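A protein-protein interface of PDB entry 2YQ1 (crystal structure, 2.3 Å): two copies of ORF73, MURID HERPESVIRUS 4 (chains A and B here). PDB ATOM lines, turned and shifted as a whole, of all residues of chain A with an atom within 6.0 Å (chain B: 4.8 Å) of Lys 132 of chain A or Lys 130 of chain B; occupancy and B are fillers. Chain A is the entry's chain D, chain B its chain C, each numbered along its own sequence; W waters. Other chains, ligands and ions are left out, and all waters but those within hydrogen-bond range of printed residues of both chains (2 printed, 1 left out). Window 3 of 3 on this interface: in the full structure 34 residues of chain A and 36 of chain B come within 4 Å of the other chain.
Printed residues of chain B within 4 Å of Lys 132 of chain A: Ile 128 (2.8 Å) and Lys 130 (3.8 Å).
Of the printed residues of chain A, Lys 130 of chain B touches Val 129 (3.4 Å), Lys 130 (2.8 Å) and Lys 132 (3.8 Å).
Of the printed residues of chain A, Phe 135 of chain B touches Val 129.
Of the printed residues of chain A, Thr 127 of chain B touches Tyr 134.
Of the printed residues of chain A, Ala 131 of chain B touches Ile 128.
Printed residues of chain A within 4 Å of Ile 128 of chain B: Ala 131 and Lys 132.
Of the printed residues of chain A, Val 129 of chain B touches Val 129 and Lys 130.
Lys 48 of chain A touches none of the printed residues of chain B.
Pro 133 of chain A touches none of the printed residues of chain B.
The nearest residue of chain B that does not touch Lys 132 of chain A is Thr 127 of chain B (4.4 Å).
The nearest residue of chain A that does not touch Lys 130 of chain B is Ile 128 of chain A (4.05 Å).
The backbone carbonyl oxygen of Ile 128 of chain B sits at hydrogen-bond distance from the backbone NH of Lys 132 of chain A (2.8 Å).
O of Ile 128 of chain A is in hydrogen-bond range of N of Lys 132 of chain B.
The backbone carbonyl oxygen (O) of Lys 130 of chain B sits at hydrogen-bond distance from the backbone NH (N) of Lys 130 of chain A, 2.8 Å away.
Among the printed residues, pairs that only touch across the chains: Ile 128 of chain A with Ala 131 of chain B, Val 129 of chain A with Val 129 of chain B, Val 129 of chain A with Lys 130 of chain B, Val 129 of chain A with Phe 135 of chain B, Lys 130 of chain A with Val 129 of chain B, Ala 131 of chain A with Ile 128 of chain B, Lys 132 of chain A with Lys 130 of chain B and Tyr 134 of chain A with Thr 127 of chain B.
The backbone carbonyl oxygen of Lys 48 of chain A is in hydrogen-bond range of the backbone NH of Ala 131 of chain A.
The backbone carbonyl oxygen (O) of Lys 48 of chain B is in hydrogen-bond range of the backbone NH (N) of Ala 131 of chain B (2.9 Å).
Of the 8 printed residues of chain A, 6 touch a printed residue of chain B.
Hydrophobic or aromatic side chains of chain A within 4 Å of the printed part of chain B: Ile 128 and Val 129.
Among the printed residues, no Asp or Glu carboxylate lies within 4 Å of a Lys or Arg side-chain nitrogen of the other chain.
Water W1 lies within hydrogen-bond range of N of Ile 128 of chain A and O of Lys 132 of chain B.
Water W2 bridges the side-chain hydroxyl (OG1) of Thr 127 of chain B (3.3 Å) and the backbone carbonyl oxygen (O) of Tyr 134 of chain A (3.5 Å).
Ile 128 of chain A touches Ala 131 of chain B, and with the chains exchanged Ala 131 of chain A touches Ile 128 of chain B.
Val 129 of chain A touches its own counterpart, Val 129 of chain B.
Val 129 of chain A touches Lys 130 of chain B, and with the chains exchanged Lys 130 of chain A touches Val 129 of chain B.
Lys 132 of chain A touches Lys 130 of chain B, but with the chains exchanged Lys 130 of chain A does not touch Lys 132 of chain B (6.3 Å).
Positions printed for both chains: 48, 128, 129, 130, 131 and 132.
Of the 11 pairs that touch across the chains among the printed residues, 8 have their exchanged pair printed and touching as well.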
ATOM      1  N   LYS A  48     -10.184  21.536   5.074  1.00  0.00           N
ATOM      2  CA  LYS A  48     -11.164  21.724   6.138  1.00  0.00           C
ATOM      3  C   LYS A  48     -12.008  20.484   6.366  1.00  0.00           C
ATOM      4  O   LYS A  48     -12.625  20.323   7.417  1.00  0.00           O
ATOM      5  CB  LYS A  48     -12.085  22.902   5.813  1.00  0.00           C
ATOM      6  CG  LYS A  48     -11.405  24.248   5.694  1.00  0.00           C
ATOM      7  CD  LYS A  48     -12.439  25.324   5.410  1.00  0.00           C
ATOM      8  CE  LYS A  48     -11.827  26.511   4.686  1.00  0.00           C
ATOM      9  NZ  LYS A  48     -12.857  27.523   4.315  1.00  0.00           N
ATOM     10  N   ILE A 128     -18.617  11.682   6.235  1.00  0.00           N
ATOM     11  CA  ILE A 128     -18.152  13.050   6.054  1.00  0.00           C
ATOM     12  C   ILE A 128     -17.617  13.570   7.365  1.00  0.00           C
ATOM     13  O   ILE A 128     -18.280  13.514   8.398  1.00  0.00           O
ATOM     14  CB  ILE A 128     -19.280  13.987   5.591  1.00  0.00           C
ATOM     15  CG1 ILE A 128     -19.831  13.550   4.232  1.00  0.00           C
ATOM     16  CG2 ILE A 128     -18.775  15.434   5.534  1.00  0.00           C
ATOM     17  CD1 ILE A 128     -18.829  13.636   3.108  1.00  0.00           C
ATOM     18  N   VAL A 129     -16.406  14.093   7.304  1.00  0.00           N
ATOM     19  CA  VAL A 129     -15.731  14.592   8.472  1.00  0.00           C
ATOM     20  C   VAL A 129     -15.346  16.064   8.287  1.00  0.00           C
ATOM     21  O   VAL A 129     -14.822  16.453   7.242  1.00  0.00           O
ATOM     22  CB  VAL A 129     -14.486  13.745   8.752  1.00  0.00           C
ATOM     23  CG1 VAL A 129     -13.692  14.323   9.838  1.00  0.00           C
ATOM     24  CG2 VAL A 129     -14.872  12.285   9.039  1.00  0.00           C
ATOM     25  N   LYS A 130     -15.596  16.879   9.309  1.00  0.00           N
ATOM     26  CA  LYS A 130     -15.279  18.301   9.241  1.00  0.00           C
ATOM     27  C   LYS A 130     -14.338  18.684  10.377  1.00  0.00           C
ATOM     28  O   LYS A 130     -14.605  18.400  11.541  1.00  0.00           O
ATOM     29  CB  LYS A 130     -16.567  19.128   9.325  1.00  0.00           C
ATOM     30  CG  LYS A 130     -16.366  20.637   9.405  1.00  0.00           C
ATOM     31  CD  LYS A 130     -15.869  21.185   8.066  1.00  0.00           C
ATOM     32  CE  LYS A 130     -15.663  22.695   8.103  1.00  0.00           C
ATOM     33  NZ  LYS A 130     -14.527  23.086   8.983  1.00  0.00           N
ATOM     34  N   ALA A 131     -13.235  19.340  10.034  1.00  0.00           N
ATOM     35  CA  ALA A 131     -12.311  19.844  11.037  1.00  0.00           C
ATOM     36  C   ALA A 131     -12.703  21.259  11.444  1.00  0.00           C
ATOM     37  O   ALA A 131     -13.106  22.068  10.608  1.00  0.00           O
ATOM     38  CB  ALA A 131     -10.893  19.819  10.515  1.00  0.00           C
ATOM     39  N   LYS A 132     -12.609  21.537  12.738  1.00  0.00           N
ATOM     40  CA  LYS A 132     -12.894  22.863  13.262  1.00  0.00           C
ATOM     41  C   LYS A 132     -11.612  23.433  13.848  1.00  0.00           C
ATOM     42  O   LYS A 132     -11.219  23.066  14.954  1.00  0.00           O
ATOM     43  CB  LYS A 132     -13.971  22.792  14.349  1.00  0.00           C
ATOM     44  CG  LYS A 132     -15.170  21.914  14.008  1.00  0.00           C
ATOM     45  CD  LYS A 132     -16.259  22.680  13.269  1.00  0.00           C
ATOM     46  CE  LYS A 132     -17.514  21.825  13.114  1.00  0.00           C
ATOM     47  NZ  LYS A 132     -18.557  22.474  12.259  1.00  0.00           N
ATOM     48  N   PRO A 133     -10.945  24.333  13.111  1.00  0.00           N
ATOM     49  CA  PRO A 133     -11.372  24.903  11.828  1.00  0.00           C
ATOM     50  C   PRO A 133     -10.723  24.278  10.587  1.00  0.00           C
ATOM     51  O   PRO A 133     -11.241  24.463   9.491  1.00  0.00           O
ATOM     52  CB  PRO A 133     -10.968  26.365  11.975  1.00  0.00           C
ATOM     53  CG  PRO A 133      -9.679  26.280  12.749  1.00  0.00           C
ATOM     54  CD  PRO A 133      -9.809  25.083  13.679  1.00  0.00           C
ATOM     55  N   TYR A 134      -9.621  23.554  10.755  1.00  0.00           N
ATOM     56  CA  TYR A 134      -8.963  22.893   9.632  1.00  0.00           C
ATOM     57  C   TYR A 134      -8.070  21.762  10.129  1.00  0.00           C
ATOM     58  O   TYR A 134      -7.752  21.688  11.316  1.00  0.00           O
ATOM     59  CB  TYR A 134      -8.128  23.892   8.818  1.00  0.00           C
ATOM     60  CG  TYR A 134      -7.081  24.620   9.632  1.00  0.00           C
ATOM     61  CD1 TYR A 134      -7.399  25.771  10.342  1.00  0.00           C
ATOM     62  CD2 TYR A 134      -5.773  24.159   9.687  1.00  0.00           C
ATOM     63  CE1 TYR A 134      -6.449  26.433  11.091  1.00  0.00           C
ATOM     64  CE2 TYR A 134      -4.812  24.817  10.431  1.00  0.00           C
ATOM     65  CZ  TYR A 134      -5.156  25.954  11.132  1.00  0.00           C
ATOM     66  OH  TYR A 134      -4.203  26.611  11.874  1.00  0.00           O
ATOM     67  N   LYS B  48     -20.052  11.399  17.943  1.00  0.00           N
ATOM     68  CA  LYS B  48     -20.224  12.361  16.860  1.00  0.00           C
ATOM     69  C   LYS B  48     -18.995  13.243  16.697  1.00  0.00           C
ATOM     70  O   LYS B  48     -18.852  13.938  15.694  1.00  0.00           O
ATOM     71  CB  LYS B  48     -21.444  13.248  17.119  1.00  0.00           C
ATOM     72  CG  LYS B  48     -22.779  12.528  17.008  1.00  0.00           C
ATOM     73  CD  LYS B  48     -23.937  13.501  17.181  1.00  0.00           C
ATOM     74  CE  LYS B  48     -25.276  12.854  16.838  1.00  0.00           C
ATOM     75  NZ  LYS B  48     -25.411  12.563  15.381  1.00  0.00           N
ATOM     76  N   SER B  49     -18.102  13.199  17.678  1.00  0.00           N
ATOM     77  CA  SER B  49     -16.974  14.117  17.703  1.00  0.00           C
ATOM     78  C   SER B  49     -15.670  13.413  18.035  1.00  0.00           C
ATOM     79  O   SER B  49     -15.659  12.256  18.450  1.00  0.00           O
ATOM     80  CB  SER B  49     -17.226  15.224  18.725  1.00  0.00           C
ATOM     81  OG  SER B  49     -18.396  15.953  18.402  1.00  0.00           O
ATOM     82  N   THR B 127      -6.848  19.057  17.283  1.00  0.00           N
ATOM     83  CA  THR B 127      -7.803  19.577  16.315  1.00  0.00           C
ATOM     84  C   THR B 127      -9.169  18.955  16.538  1.00  0.00           C
ATOM     85  O   THR B 127      -9.327  17.745  16.404  1.00  0.00           O
ATOM     86  CB  THR B 127      -7.365  19.256  14.884  1.00  0.00           C
ATOM     87  OG1 THR B 127      -6.029  19.730  14.673  1.00  0.00           O
ATOM     88  CG2 THR B 127      -8.317  19.899  13.883  1.00  0.00           C
ATOM     89  N   ILE B 128     -10.154  19.785  16.879  1.00  0.00           N
ATOM     90  CA  ILE B 128     -11.516  19.313  17.043  1.00  0.00           C
ATOM     91  C   ILE B 128     -12.051  18.868  15.698  1.00  0.00           C
ATOM     92  O   ILE B 128     -11.967  19.582  14.685  1.00  0.00           O
ATOM     93  CB  ILE B 128     -12.421  20.417  17.589  1.00  0.00           C
ATOM     94  CG1 ILE B 128     -11.918  20.891  18.957  1.00  0.00           C
ATOM     95  CG2 ILE B 128     -13.864  19.927  17.655  1.00  0.00           C
ATOM     96  CD1 ILE B 128     -11.856  19.804  20.015  1.00  0.00           C
ATOM     97  N   VAL B 129     -12.615  17.668  15.708  1.00  0.00           N
ATOM     98  CA  VAL B 129     -13.196  17.078  14.516  1.00  0.00           C
ATOM     99  C   VAL B 129     -14.636  16.632  14.760  1.00  0.00           C
ATOM    100  O   VAL B 129     -14.990  16.244  15.871  1.00  0.00           O
ATOM    101  CB  VAL B 129     -12.327  15.885  14.017  1.00  0.00           C
ATOM    102  CG1 VAL B 129     -12.906  15.257  12.808  1.00  0.00           C
ATOM    103  CG2 VAL B 129     -10.857  16.337  13.792  1.00  0.00           C
ATOM    104  N   LYS B 130     -15.461  16.664  13.720  1.00  0.00           N
ATOM    105  CA  LYS B 130     -16.871  16.326  13.844  1.00  0.00           C
ATOM    106  C   LYS B 130     -17.303  15.449  12.666  1.00  0.00           C
ATOM    107  O   LYS B 130     -16.860  15.650  11.531  1.00  0.00           O
ATOM    108  CB  LYS B 130     -17.686  17.617  13.900  1.00  0.00           C
ATOM    109  CG  LYS B 130     -19.160  17.494  13.632  1.00  0.00           C
ATOM    110  CD  LYS B 130     -19.807  18.862  13.788  1.00  0.00           C
ATOM    111  CE  LYS B 130     -21.234  18.889  13.263  1.00  0.00           C
ATOM    112  NZ  LYS B 130     -21.966  20.109  13.715  1.00  0.00           N
ATOM    113  N   ALA B 131     -18.156  14.469  12.947  1.00  0.00           N
ATOM    114  CA  ALA B 131     -18.666  13.563  11.925  1.00  0.00           C
ATOM    115  C   ALA B 131     -20.180  13.672  11.780  1.00  0.00           C
ATOM    116  O   ALA B 131     -20.885  14.032  12.726  1.00  0.00           O
ATOM    117  CB  ALA B 131     -18.270  12.131  12.244  1.00  0.00           C
ATOM    118  N   LYS B 132     -20.669  13.367  10.582  1.00  0.00           N
ATOM    119  CA  LYS B 132     -22.105  13.356  10.329  1.00  0.00           C
ATOM    120  C   LYS B 132     -22.563  12.015   9.745  1.00  0.00           C
ATOM    121  O   LYS B 132     -22.029  11.553   8.735  1.00  0.00           O
ATOM    122  CB  LYS B 132     -22.501  14.520   9.409  1.00  0.00           C
ATOM    123  CG  LYS B 132     -21.835  14.521   8.041  1.00  0.00           C
ATOM    124  CD  LYS B 132     -22.439  15.590   7.142  1.00  0.00           C
ATOM    125  CE  LYS B 132     -23.963  15.549   7.185  1.00  0.00           C
ATOM    126  NZ  LYS B 132     -24.560  16.820   6.690  1.00  0.00           N
ATOM    127  N   PHE B 135     -19.332   9.096  13.963  1.00  0.00           N
ATOM    128  CA  PHE B 135     -18.255   8.210  13.538  1.00  0.00           C
ATOM    129  C   PHE B 135     -18.635   6.720  13.574  1.00  0.00           C
ATOM    130  O   PHE B 135     -19.289   6.259  14.515  1.00  0.00           O
ATOM    131  CB  PHE B 135     -17.003   8.450  14.394  1.00  0.00           C
ATOM    132  CG  PHE B 135     -16.306   9.754  14.118  1.00  0.00           C
ATOM    133  CD1 PHE B 135     -15.476   9.894  13.016  1.00  0.00           C
ATOM    134  CD2 PHE B 135     -16.446  10.828  14.987  1.00  0.00           C
ATOM    135  CE1 PHE B 135     -14.825  11.093  12.768  1.00  0.00           C
ATOM    136  CE2 PHE B 135     -15.798  12.026  14.747  1.00  0.00           C
ATOM    137  CZ  PHE B 135     -14.985  12.159  13.636  1.00  0.00           C
HETATM  138  O   HOH W   1     -21.241  11.035   5.925  1.00  0.00           O
HETATM  139  O   HOH W   2      -5.063  22.546  13.308  1.00  0.00           O
